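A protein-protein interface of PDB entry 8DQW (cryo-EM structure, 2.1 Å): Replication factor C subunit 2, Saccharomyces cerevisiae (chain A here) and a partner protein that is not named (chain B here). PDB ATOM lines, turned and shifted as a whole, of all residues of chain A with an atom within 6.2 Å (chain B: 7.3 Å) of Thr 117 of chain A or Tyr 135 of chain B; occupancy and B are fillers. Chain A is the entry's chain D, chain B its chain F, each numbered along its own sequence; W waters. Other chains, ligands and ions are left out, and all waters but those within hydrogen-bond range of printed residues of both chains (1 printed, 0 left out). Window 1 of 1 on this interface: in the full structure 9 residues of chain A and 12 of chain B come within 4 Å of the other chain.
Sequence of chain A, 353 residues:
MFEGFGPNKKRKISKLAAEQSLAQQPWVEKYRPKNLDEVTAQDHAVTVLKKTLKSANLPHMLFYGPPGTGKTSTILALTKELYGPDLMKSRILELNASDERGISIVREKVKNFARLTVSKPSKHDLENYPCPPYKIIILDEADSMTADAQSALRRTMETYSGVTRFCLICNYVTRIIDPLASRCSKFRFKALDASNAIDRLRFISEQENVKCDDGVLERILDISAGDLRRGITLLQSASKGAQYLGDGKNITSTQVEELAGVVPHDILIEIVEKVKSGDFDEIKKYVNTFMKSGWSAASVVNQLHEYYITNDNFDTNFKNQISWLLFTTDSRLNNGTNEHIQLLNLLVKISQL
OD1 of Asn 112 of chain A is in hydrogen-bond range of NZ of Lys 85 of chain B (3.4 Å). The guanidinium group (NH1) of Arg 115 of chain A is in salt-bridge range of the side-chain carboxylate (OD1) of Asp 36 of chain B, at 2.9 Å. The guanidinium group (NH2) of Arg 115 of chain A lies within hydrogen-bond range of the side-chain sulfur (SG) of Cys 83 of chain B (3.6 Å). The guanidinium group of Arg 115 of chain A is in hydrogen-bond range of the backbone carbonyl oxygen of Leu 136 of chain B. OG1 of Thr 117 of chain A is in hydrogen-bond range of OG1 of Thr 134 of chain B, at 2.5 Å.
The side-chain hydroxyl (OG) of Ser 90 of chain A sits at hydrogen-bond distance from the side-chain hydroxyl (OG) of Ser 119 of chain A, at 2.8 Å. NZ of Lys 135 of chain A sits at hydrogen-bond distance from O of Leu 116 of chain A (2.5 Å). O of Val 163 of chain A lies within hydrogen-bond range of N of Lys 135 of chain A (2.7 Å). The side-chain sulfur (SG) of Cys 83 of chain B is in hydrogen-bond range of the side-chain carboxylate (OD2) of Asp 36 of chain B (3.1 Å). The backbone NH of Tyr 135 of chain B lies within hydrogen-bond range of the backbone carbonyl oxygen of Cys 83 of chain B. N of His 113 of chain B is in hydrogen-bond range of OH of Tyr 110 of chain B.
Asn 112 of chain A touches Tyr 135 of chain B (O to CE2, 3.6 Å). Arg 115 of chain A touches Tyr 135 of chain B (O to CA, 3.6 Å). Arg 115 of chain A touches Lys 138 of chain B (NH2 to CG, 3.9 Å). CB of Ser 133 of chain B touches CD1 of Leu 116 of chain A, 3.7 Å away. CD1 of Leu 116 of chain A touches CE2 of Tyr 135 of chain B (3.6 Å). Thr 117 of chain A touches His 113 of chain B. Tyr 135 of chain B touches Thr 117 of chain A. CG2 of Thr 117 of chain A touches N of Leu 136 of chain B, at 3.9 Å. O of Val 118 of chain A touches CA of Gly 114 of chain B, at 3.3 Å. Leu 136 of chain B touches Val 163 of chain A (CD1 to CG2, 3.6 Å).
Tyr 135 of chain B touches just these residues of chain A: Asn 112, Arg 115, Leu 116 and Thr 117. Of the printed residues of chain A, Leu 136 of chain B touches Arg 115, Thr 117 and Val 163. Of the printed residues of chain A, Lys 85 of chain B touches Asn 112 (3.4 Å). Of the printed residues of chain B, Ser 119 of chain A touches Gly 114. Of the printed residues of chain B, Val 118 of chain A touches Gly 114 (3.3 Å). Printed residues of chain A within 4 Å of His 113 of chain B: Thr 117. Lys 135 of chain A touches none of the printed residues of chain B. The nearest printed residue of chain A that does not touch Leu 136 of chain B is Leu 116 of chain A (4.8 Å).
Printed residues of chain B that touch a printed residue of chain A: Asp 36, Cys 83, Lys 85, His 113, Gly 114, Ser 133, Thr 134, Tyr 135, Leu 136 and Lys 138. Of the 11 printed residues of chain A, 7 touch a printed residue of chain B. Hydrophobic or aromatic side chains of chain A within 4 Å of the printed part of chain B: Leu 116 and Val 163. Along chain A the printed residues that touch a printed residue of chain B span positions 112 to 163. Among the printed residues, 17 pairs touch across the chains. Among the printed residues, Asp or Glu carboxylates within 4 Å of a Lys or Arg side-chain nitrogen of the other chain: Arg 115 of chain A with Asp 36 of chain B (2.9 Å).
Water W1 lies within hydrogen-bond range of ND1 of His 113 of chain B, O of Val 118 of chain A and N of Gly 114 of chain B.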
ATOM      1  N   SER A  90      14.238  -4.475 -17.367  1.00  0.00           N
ATOM      2  CA  SER A  90      13.179  -4.228 -18.337  1.00  0.00           C
ATOM      3  C   SER A  90      12.704  -2.780 -18.355  1.00  0.00           C
ATOM      4  O   SER A  90      11.900  -2.425 -19.223  1.00  0.00           O
ATOM      5  CB  SER A  90      11.982  -5.147 -18.058  1.00  0.00           C
ATOM      6  OG  SER A  90      11.208  -4.660 -16.977  1.00  0.00           O
ATOM      7  N   LYS A 111      13.578   6.134 -29.658  1.00  0.00           N
ATOM      8  CA  LYS A 111      12.140   6.316 -29.830  1.00  0.00           C
ATOM      9  C   LYS A 111      11.380   5.019 -29.579  1.00  0.00           C
ATOM     10  O   LYS A 111      10.339   5.023 -28.909  1.00  0.00           O
ATOM     11  CB  LYS A 111      11.841   6.844 -31.234  1.00  0.00           C
ATOM     12  CG  LYS A 111      10.638   7.772 -31.295  1.00  0.00           C
ATOM     13  CD  LYS A 111      10.067   7.863 -32.703  1.00  0.00           C
ATOM     14  CE  LYS A 111      10.212   9.261 -33.283  1.00  0.00           C
ATOM     15  NZ  LYS A 111       9.208   9.523 -34.351  1.00  0.00           N
ATOM     16  N   ASN A 112      11.881   3.897 -30.104  1.00  0.00           N
ATOM     17  CA  ASN A 112      11.206   2.623 -29.886  1.00  0.00           C
ATOM     18  C   ASN A 112      11.147   2.280 -28.407  1.00  0.00           C
ATOM     19  O   ASN A 112      10.103   1.848 -27.905  1.00  0.00           O
ATOM     20  CB  ASN A 112      11.915   1.516 -30.665  1.00  0.00           C
ATOM     21  CG  ASN A 112      11.770   1.674 -32.164  1.00  0.00           C
ATOM     22  OD1 ASN A 112      11.045   2.547 -32.639  1.00  0.00           O
ATOM     23  ND2 ASN A 112      12.468   0.834 -32.918  1.00  0.00           N
ATOM     24  N   PHE A 113      12.256   2.468 -27.686  1.00  0.00           N
ATOM     25  CA  PHE A 113      12.225   2.206 -26.251  1.00  0.00           C
ATOM     26  C   PHE A 113      11.257   3.145 -25.539  1.00  0.00           C
ATOM     27  O   PHE A 113      10.514   2.721 -24.648  1.00  0.00           O
ATOM     28  CB  PHE A 113      13.622   2.332 -25.648  1.00  0.00           C
ATOM     29  CG  PHE A 113      13.717   1.790 -24.250  1.00  0.00           C
ATOM     30  CD1 PHE A 113      13.847   0.429 -24.025  1.00  0.00           C
ATOM     31  CD2 PHE A 113      13.655   2.640 -23.160  1.00  0.00           C
ATOM     32  CE1 PHE A 113      13.926  -0.070 -22.738  1.00  0.00           C
ATOM     33  CE2 PHE A 113      13.733   2.147 -21.871  1.00  0.00           C
ATOM     34  CZ  PHE A 113      13.869   0.791 -21.661  1.00  0.00           C
ATOM     35  N   ARG A 115       8.582   4.418 -26.657  1.00  0.00           N
ATOM     36  CA  ARG A 115       7.219   4.022 -26.981  1.00  0.00           C
ATOM     37  C   ARG A 115       6.853   2.640 -26.448  1.00  0.00           C
ATOM     38  O   ARG A 115       5.683   2.254 -26.526  1.00  0.00           O
ATOM     39  CB  ARG A 115       7.022   4.055 -28.501  1.00  0.00           C
ATOM     40  CG  ARG A 115       5.577   3.920 -28.948  1.00  0.00           C
ATOM     41  CD  ARG A 115       5.463   3.980 -30.458  1.00  0.00           C
ATOM     42  NE  ARG A 115       4.145   3.555 -30.914  1.00  0.00           N
ATOM     43  CZ  ARG A 115       3.894   3.034 -32.107  1.00  0.00           C
ATOM     44  NH1 ARG A 115       4.849   2.877 -33.009  1.00  0.00           N
ATOM     45  NH2 ARG A 115       2.653   2.663 -32.403  1.00  0.00           N
ATOM     46  N   LEU A 116       7.814   1.901 -25.899  1.00  0.00           N
ATOM     47  CA  LEU A 116       7.549   0.546 -25.434  1.00  0.00           C
ATOM     48  C   LEU A 116       6.531   0.549 -24.300  1.00  0.00           C
ATOM     49  O   LEU A 116       6.525   1.441 -23.447  1.00  0.00           O
ATOM     50  CB  LEU A 116       8.850  -0.107 -24.962  1.00  0.00           C
ATOM     51  CG  LEU A 116       8.835  -1.627 -24.794  1.00  0.00           C
ATOM     52  CD1 LEU A 116       8.877  -2.320 -26.146  1.00  0.00           C
ATOM     53  CD2 LEU A 116       9.994  -2.080 -23.920  1.00  0.00           C
ATOM     54  N   THR A 117       5.661  -0.458 -24.293  1.00  0.00           N
ATOM     55  CA  THR A 117       4.698  -0.597 -23.211  1.00  0.00           C
ATOM     56  C   THR A 117       5.418  -0.886 -21.897  1.00  0.00           C
ATOM     57  O   THR A 117       6.453  -1.558 -21.863  1.00  0.00           O
ATOM     58  CB  THR A 117       3.698  -1.717 -23.510  1.00  0.00           C
ATOM     59  OG1 THR A 117       4.388  -2.867 -24.011  1.00  0.00           O
ATOM     60  CG2 THR A 117       2.671  -1.256 -24.536  1.00  0.00           C
ATOM     61  N   VAL A 118       4.862  -0.362 -20.806  1.00  0.00           N
ATOM     62  CA  VAL A 118       5.462  -0.557 -19.491  1.00  0.00           C
ATOM     63  C   VAL A 118       5.314  -2.016 -19.083  1.00  0.00           C
ATOM     64  O   VAL A 118       4.207  -2.571 -19.085  1.00  0.00           O
ATOM     65  CB  VAL A 118       4.819   0.384 -18.461  1.00  0.00           C
ATOM     66  CG1 VAL A 118       5.495   0.231 -17.108  1.00  0.00           C
ATOM     67  CG2 VAL A 118       4.900   1.830 -18.938  1.00  0.00           C
ATOM     68  N   SER A 119       6.430  -2.644 -18.726  1.00  0.00           N
ATOM     69  CA  SER A 119       6.425  -4.064 -18.403  1.00  0.00           C
ATOM     70  C   SER A 119       5.660  -4.326 -17.111  1.00  0.00           C
ATOM     71  O   SER A 119       5.596  -3.481 -16.214  1.00  0.00           O
ATOM     72  CB  SER A 119       7.856  -4.588 -18.275  1.00  0.00           C
ATOM     73  OG  SER A 119       8.568  -3.889 -17.269  1.00  0.00           O
ATOM     74  N   LYS A 135       9.263   3.924 -17.536  1.00  0.00           N
ATOM     75  CA  LYS A 135      10.639   3.497 -17.734  1.00  0.00           C
ATOM     76  C   LYS A 135      11.570   4.702 -17.617  1.00  0.00           C
ATOM     77  O   LYS A 135      11.136   5.842 -17.440  1.00  0.00           O
ATOM     78  CB  LYS A 135      10.809   2.809 -19.092  1.00  0.00           C
ATOM     79  CG  LYS A 135       9.669   1.883 -19.509  1.00  0.00           C
ATOM     80  CD  LYS A 135       9.475   1.905 -21.020  1.00  0.00           C
ATOM     81  CE  LYS A 135       8.598   3.071 -21.446  1.00  0.00           C
ATOM     82  NZ  LYS A 135       8.318   3.067 -22.905  1.00  0.00           N
ATOM     83  N   VAL A 163       4.956   7.381 -20.050  1.00  0.00           N
ATOM     84  CA  VAL A 163       5.489   6.047 -19.795  1.00  0.00           C
ATOM     85  C   VAL A 163       7.013   6.065 -19.748  1.00  0.00           C
ATOM     86  O   VAL A 163       7.640   5.057 -19.404  1.00  0.00           O
ATOM     87  CB  VAL A 163       4.995   5.045 -20.858  1.00  0.00           C
ATOM     88  CG1 VAL A 163       3.492   4.837 -20.734  1.00  0.00           C
ATOM     89  CG2 VAL A 163       5.367   5.516 -22.261  1.00  0.00           C
ATOM     90  N   ASP B  36       4.127  -0.556 -37.981  1.00  0.00           N
ATOM     91  CA  ASP B  36       3.369  -1.113 -36.871  1.00  0.00           C
ATOM     92  C   ASP B  36       2.104  -1.812 -37.360  1.00  0.00           C
ATOM     93  O   ASP B  36       1.552  -1.482 -38.411  1.00  0.00           O
ATOM     94  CB  ASP B  36       2.996  -0.018 -35.873  1.00  0.00           C
ATOM     95  CG  ASP B  36       4.185   0.465 -35.068  1.00  0.00           C
ATOM     96  OD1 ASP B  36       4.897   1.373 -35.546  1.00  0.00           O
ATOM     97  OD2 ASP B  36       4.412  -0.064 -33.960  1.00  0.00           O
ATOM     98  N   LEU B  38      -1.671  -3.241 -35.583  1.00  0.00           N
ATOM     99  CA  LEU B  38      -2.556  -3.273 -34.429  1.00  0.00           C
ATOM    100  C   LEU B  38      -3.280  -4.612 -34.399  1.00  0.00           C
ATOM    101  O   LEU B  38      -3.766  -5.082 -35.430  1.00  0.00           O
ATOM    102  CB  LEU B  38      -3.567  -2.126 -34.482  1.00  0.00           C
ATOM    103  CG  LEU B  38      -3.203  -0.831 -33.748  1.00  0.00           C
ATOM    104  CD1 LEU B  38      -1.732  -0.473 -33.925  1.00  0.00           C
ATOM    105  CD2 LEU B  38      -4.091   0.310 -34.223  1.00  0.00           C
ATOM    106  N   LYS B  81      -6.508  -4.424 -27.071  1.00  0.00           N
ATOM    107  CA  LYS B  81      -5.806  -3.758 -28.160  1.00  0.00           C
ATOM    108  C   LYS B  81      -4.311  -3.796 -27.882  1.00  0.00           C
ATOM    109  O   LYS B  81      -3.881  -3.488 -26.765  1.00  0.00           O
ATOM    110  CB  LYS B  81      -6.267  -2.304 -28.300  1.00  0.00           C
ATOM    111  CG  LYS B  81      -7.599  -2.119 -29.011  1.00  0.00           C
ATOM    112  CD  LYS B  81      -7.689  -0.747 -29.676  1.00  0.00           C
ATOM    113  CE  LYS B  81      -7.610   0.413 -28.684  1.00  0.00           C
ATOM    114  NZ  LYS B  81      -8.093   0.088 -27.310  1.00  0.00           N
ATOM    115  N   LEU B  82      -3.521  -4.168 -28.887  1.00  0.00           N
ATOM    116  CA  LEU B  82      -2.072  -4.122 -28.736  1.00  0.00           C
ATOM    117  C   LEU B  82      -1.440  -3.733 -30.063  1.00  0.00           C
ATOM    118  O   LEU B  82      -2.082  -3.774 -31.113  1.00  0.00           O
ATOM    119  CB  LEU B  82      -1.506  -5.458 -28.231  1.00  0.00           C
ATOM    120  CG  LEU B  82      -1.653  -6.678 -29.140  1.00  0.00           C
ATOM    121  CD1 LEU B  82      -0.445  -7.589 -29.011  1.00  0.00           C
ATOM    122  CD2 LEU B  82      -2.933  -7.434 -28.819  1.00  0.00           C
ATOM    123  N   CYS B  83      -0.171  -3.337 -30.003  1.00  0.00           N
ATOM    124  CA  CYS B  83       0.578  -2.911 -31.178  1.00  0.00           C
ATOM    125  C   CYS B  83       1.912  -3.639 -31.216  1.00  0.00           C
ATOM    126  O   CYS B  83       2.611  -3.708 -30.200  1.00  0.00           O
ATOM    127  CB  CYS B  83       0.803  -1.395 -31.167  1.00  0.00           C
ATOM    128  SG  CYS B  83       1.758  -0.782 -32.567  1.00  0.00           S
ATOM    129  N   VAL B  84       2.266  -4.172 -32.386  1.00  0.00           N
ATOM    130  CA  VAL B  84       3.519  -4.890 -32.577  1.00  0.00           C
ATOM    131  C   VAL B  84       4.184  -4.377 -33.847  1.00  0.00           C
ATOM    132  O   VAL B  84       3.600  -3.619 -34.620  1.00  0.00           O
ATOM    133  CB  VAL B  84       3.315  -6.419 -32.650  1.00  0.00           C
ATOM    134  CG1 VAL B  84       3.065  -6.986 -31.260  1.00  0.00           C
ATOM    135  CG2 VAL B  84       2.165  -6.763 -33.583  1.00  0.00           C
ATOM    136  N   LYS B  85       5.431  -4.795 -34.050  1.00  0.00           N
ATOM    137  CA  LYS B  85       6.205  -4.416 -35.224  1.00  0.00           C
ATOM    138  C   LYS B  85       6.129  -5.527 -36.263  1.00  0.00           C
ATOM    139  O   LYS B  85       6.411  -6.690 -35.956  1.00  0.00           O
ATOM    140  CB  LYS B  85       7.663  -4.135 -34.854  1.00  0.00           C
ATOM    141  CG  LYS B  85       7.855  -2.932 -33.941  1.00  0.00           C
ATOM    142  CD  LYS B  85       7.543  -1.625 -34.656  1.00  0.00           C
ATOM    143  CE  LYS B  85       7.531  -0.452 -33.688  1.00  0.00           C
ATOM    144  NZ  LYS B  85       8.903  -0.052 -33.276  1.00  0.00           N
ATOM    145  N   HIS B  88       9.403  -7.661 -36.991  1.00  0.00           N
ATOM    146  CA  HIS B  88       9.720  -8.710 -36.027  1.00  0.00           C
ATOM    147  C   HIS B  88       8.964  -9.994 -36.349  1.00  0.00           C
ATOM    148  O   HIS B  88       9.559 -11.075 -36.443  1.00  0.00           O
ATOM    149  CB  HIS B  88       9.387  -8.239 -34.610  1.00  0.00           C
ATOM    150  CG  HIS B  88      10.195  -7.062 -34.158  1.00  0.00           C
ATOM    151  ND1 HIS B  88       9.924  -6.381 -32.991  1.00  0.00           N
ATOM    152  CD2 HIS B  88      11.265  -6.446 -34.714  1.00  0.00           C
ATOM    153  CE1 HIS B  88      10.792  -5.396 -32.848  1.00  0.00           C
ATOM    154  NE2 HIS B  88      11.617  -5.414 -33.879  1.00  0.00           N
ATOM    155  N   TYR B 110      -1.883 -14.068 -25.235  1.00  0.00           N
ATOM    156  CA  TYR B 110      -1.708 -12.712 -24.736  1.00  0.00           C
ATOM    157  C   TYR B 110      -2.276 -12.632 -23.327  1.00  0.00           C
ATOM    158  O   TYR B 110      -3.333 -13.205 -23.047  1.00  0.00           O
ATOM    159  CB  TYR B 110      -2.393 -11.689 -25.652  1.00  0.00           C
ATOM    160  CG  TYR B 110      -2.146 -10.249 -25.265  1.00  0.00           C
ATOM    161  CD1 TYR B 110      -0.856  -9.759 -25.118  1.00  0.00           C
ATOM    162  CD2 TYR B 110      -3.206  -9.378 -25.049  1.00  0.00           C
ATOM    163  CE1 TYR B 110      -0.627  -8.443 -24.767  1.00  0.00           C
ATOM    164  CE2 TYR B 110      -2.988  -8.060 -24.698  1.00  0.00           C
ATOM    165  CZ  TYR B 110      -1.697  -7.598 -24.559  1.00  0.00           C
ATOM    166  OH  TYR B 110      -1.475  -6.287 -24.209  1.00  0.00           O
ATOM    167  N   HIS B 113      -2.359  -5.926 -21.127  1.00  0.00           N
ATOM    168  CA  HIS B 113      -1.415  -4.823 -21.250  1.00  0.00           C
ATOM    169  C   HIS B 113      -0.214  -5.043 -20.338  1.00  0.00           C
ATOM    170  O   HIS B 113      -0.355  -5.453 -19.183  1.00  0.00           O
ATOM    171  CB  HIS B 113      -2.105  -3.501 -20.906  1.00  0.00           C
ATOM    172  CG  HIS B 113      -1.488  -2.305 -21.562  1.00  0.00           C
ATOM    173  ND1 HIS B 113      -1.021  -1.223 -20.846  1.00  0.00           N
ATOM    174  CD2 HIS B 113      -1.263  -2.019 -22.865  1.00  0.00           C
ATOM    175  CE1 HIS B 113      -0.535  -0.323 -21.681  1.00  0.00           C
ATOM    176  NE2 HIS B 113      -0.668  -0.781 -22.912  1.00  0.00           N
ATOM    177  N   GLY B 114       0.977  -4.767 -20.868  1.00  0.00           N
ATOM    178  CA  GLY B 114       2.209  -4.956 -20.135  1.00  0.00           C
ATOM    179  C   GLY B 114       2.897  -6.285 -20.366  1.00  0.00           C
ATOM    180  O   GLY B 114       4.013  -6.479 -19.866  1.00  0.00           O
ATOM    181  N   SER B 115       2.277  -7.200 -21.099  1.00  0.00           N
ATOM    182  CA  SER B 115       2.842  -8.502 -21.409  1.00  0.00           C
ATOM    183  C   SER B 115       3.076  -8.622 -22.909  1.00  0.00           C
ATOM    184  O   SER B 115       2.417  -7.944 -23.705  1.00  0.00           O
ATOM    185  CB  SER B 115       1.914  -9.632 -20.939  1.00  0.00           C
ATOM    186  OG  SER B 115       0.586  -9.418 -21.387  1.00  0.00           O
ATOM    187  N   PRO B 116       4.009  -9.472 -23.330  1.00  0.00           N
ATOM    188  CA  PRO B 116       4.278  -9.625 -24.761  1.00  0.00           C
ATOM    189  C   PRO B 116       3.220 -10.472 -25.454  1.00  0.00           C
ATOM    190  O   PRO B 116       2.449 -11.199 -24.827  1.00  0.00           O
ATOM    191  CB  PRO B 116       5.642 -10.322 -24.789  1.00  0.00           C
ATOM    192  CG  PRO B 116       5.670 -11.119 -23.531  1.00  0.00           C
ATOM    193  CD  PRO B 116       4.859 -10.356 -22.511  1.00  0.00           C
ATOM    194  N   TYR B 132       6.840 -11.208 -28.639  1.00  0.00           N
ATOM    195  CA  TYR B 132       6.985  -9.916 -29.292  1.00  0.00           C
ATOM    196  C   TYR B 132       6.620  -8.814 -28.310  1.00  0.00           C
ATOM    197  O   TYR B 132       5.542  -8.843 -27.707  1.00  0.00           O
ATOM    198  CB  TYR B 132       6.095  -9.826 -30.532  1.00  0.00           C
ATOM    199  CG  TYR B 132       6.292 -10.952 -31.518  1.00  0.00           C
ATOM    200  CD1 TYR B 132       7.439 -11.030 -32.295  1.00  0.00           C
ATOM    201  CD2 TYR B 132       5.328 -11.939 -31.672  1.00  0.00           C
ATOM    202  CE1 TYR B 132       7.621 -12.055 -33.198  1.00  0.00           C
ATOM    203  CE2 TYR B 132       5.501 -12.970 -32.574  1.00  0.00           C
ATOM    204  CZ  TYR B 132       6.649 -13.024 -33.334  1.00  0.00           C
ATOM    205  OH  TYR B 132       6.825 -14.049 -34.233  1.00  0.00           O
ATOM    206  N   SER B 133       7.525  -7.853 -28.148  1.00  0.00           N
ATOM    207  CA  SER B 133       7.248  -6.695 -27.315  1.00  0.00           C
ATOM    208  C   SER B 133       6.155  -5.840 -27.946  1.00  0.00           C
ATOM    209  O   SER B 133       6.037  -5.744 -29.170  1.00  0.00           O
ATOM    210  CB  SER B 133       8.514  -5.862 -27.118  1.00  0.00           C
ATOM    211  OG  SER B 133       9.592  -6.666 -26.669  1.00  0.00           O
ATOM    212  N   THR B 134       5.347  -5.220 -27.093  1.00  0.00           N
ATOM    213  CA  THR B 134       4.235  -4.386 -27.521  1.00  0.00           C
ATOM    214  C   THR B 134       4.558  -2.916 -27.281  1.00  0.00           C
ATOM    215  O   THR B 134       5.400  -2.568 -26.450  1.00  0.00           O
ATOM    216  CB  THR B 134       2.947  -4.771 -26.783  1.00  0.00           C
ATOM    217  OG1 THR B 134       3.120  -4.576 -25.375  1.00  0.00           O
ATOM    218  CG2 THR B 134       2.591  -6.227 -27.051  1.00  0.00           C
ATOM    219  N   TYR B 135       3.869  -2.053 -28.024  1.00  0.00           N
ATOM    220  CA  TYR B 135       4.119  -0.620 -28.003  1.00  0.00           C
ATOM    221  C   TYR B 135       2.806   0.132 -27.830  1.00  0.00           C
ATOM    222  O   TYR B 135       1.724  -0.395 -28.098  1.00  0.00           O
ATOM    223  CB  TYR B 135       4.819  -0.156 -29.289  1.00  0.00           C
ATOM    224  CG  TYR B 135       6.119  -0.877 -29.573  1.00  0.00           C
ATOM    225  CD1 TYR B 135       6.124  -2.132 -30.164  1.00  0.00           C
ATOM    226  CD2 TYR B 135       7.340  -0.299 -29.249  1.00  0.00           C
ATOM    227  CE1 TYR B 135       7.309  -2.795 -30.425  1.00  0.00           C
ATOM    228  CE2 TYR B 135       8.528  -0.953 -29.507  1.00  0.00           C
ATOM    229  CZ  TYR B 135       8.508  -2.201 -30.094  1.00  0.00           C
ATOM    230  OH  TYR B 135       9.691  -2.854 -30.351  1.00  0.00           O
ATOM    231  N   LEU B 136       2.914   1.375 -27.368  1.00  0.00           N
ATOM    232  CA  LEU B 136       1.736   2.220 -27.228  1.00  0.00           C
ATOM    233  C   LEU B 136       1.098   2.463 -28.590  1.00  0.00           C
ATOM    234  O   LEU B 136       1.788   2.587 -29.606  1.00  0.00           O
ATOM    235  CB  LEU B 136       2.108   3.554 -26.580  1.00  0.00           C
ATOM    236  CG  LEU B 136       2.583   3.524 -25.125  1.00  0.00           C
ATOM    237  CD1 LEU B 136       2.665   4.940 -24.578  1.00  0.00           C
ATOM    238  CD2 LEU B 136       1.675   2.665 -24.256  1.00  0.00           C
ATOM    239  N   ILE B 137      -0.226   2.531 -28.607  1.00  0.00           N
ATOM    240  CA  ILE B 137      -0.986   2.709 -29.839  1.00  0.00           C
ATOM    241  C   ILE B 137      -1.072   4.193 -30.163  1.00  0.00           C
ATOM    242  O   ILE B 137      -1.328   5.026 -29.285  1.00  0.00           O
ATOM    243  CB  ILE B 137      -2.385   2.079 -29.711  1.00  0.00           C
ATOM    244  CG1 ILE B 137      -2.267   0.556 -29.593  1.00  0.00           C
ATOM    245  CG2 ILE B 137      -3.249   2.455 -30.905  1.00  0.00           C
ATOM    246  CD1 ILE B 137      -3.472  -0.106 -28.974  1.00  0.00           C
ATOM    247  N   LYS B 138      -0.865   4.524 -31.435  1.00  0.00           N
ATOM    248  CA  LYS B 138      -0.858   5.916 -31.863  1.00  0.00           C
ATOM    249  C   LYS B 138      -2.234   6.549 -31.685  1.00  0.00           C
ATOM    250  O   LYS B 138      -3.268   5.879 -31.755  1.00  0.00           O
ATOM    251  CB  LYS B 138      -0.425   6.019 -33.326  1.00  0.00           C
ATOM    252  CG  LYS B 138       1.081   6.044 -33.523  1.00  0.00           C
ATOM    253  CD  LYS B 138       1.646   7.441 -33.326  1.00  0.00           C
ATOM    254  CE  LYS B 138       3.015   7.398 -32.668  1.00  0.00           C
ATOM    255  NZ  LYS B 138       4.022   6.696 -33.509  1.00  0.00           N
HETATM  256  O   HOH W   1       1.343  -1.658 -19.578  1.00  0.00           O
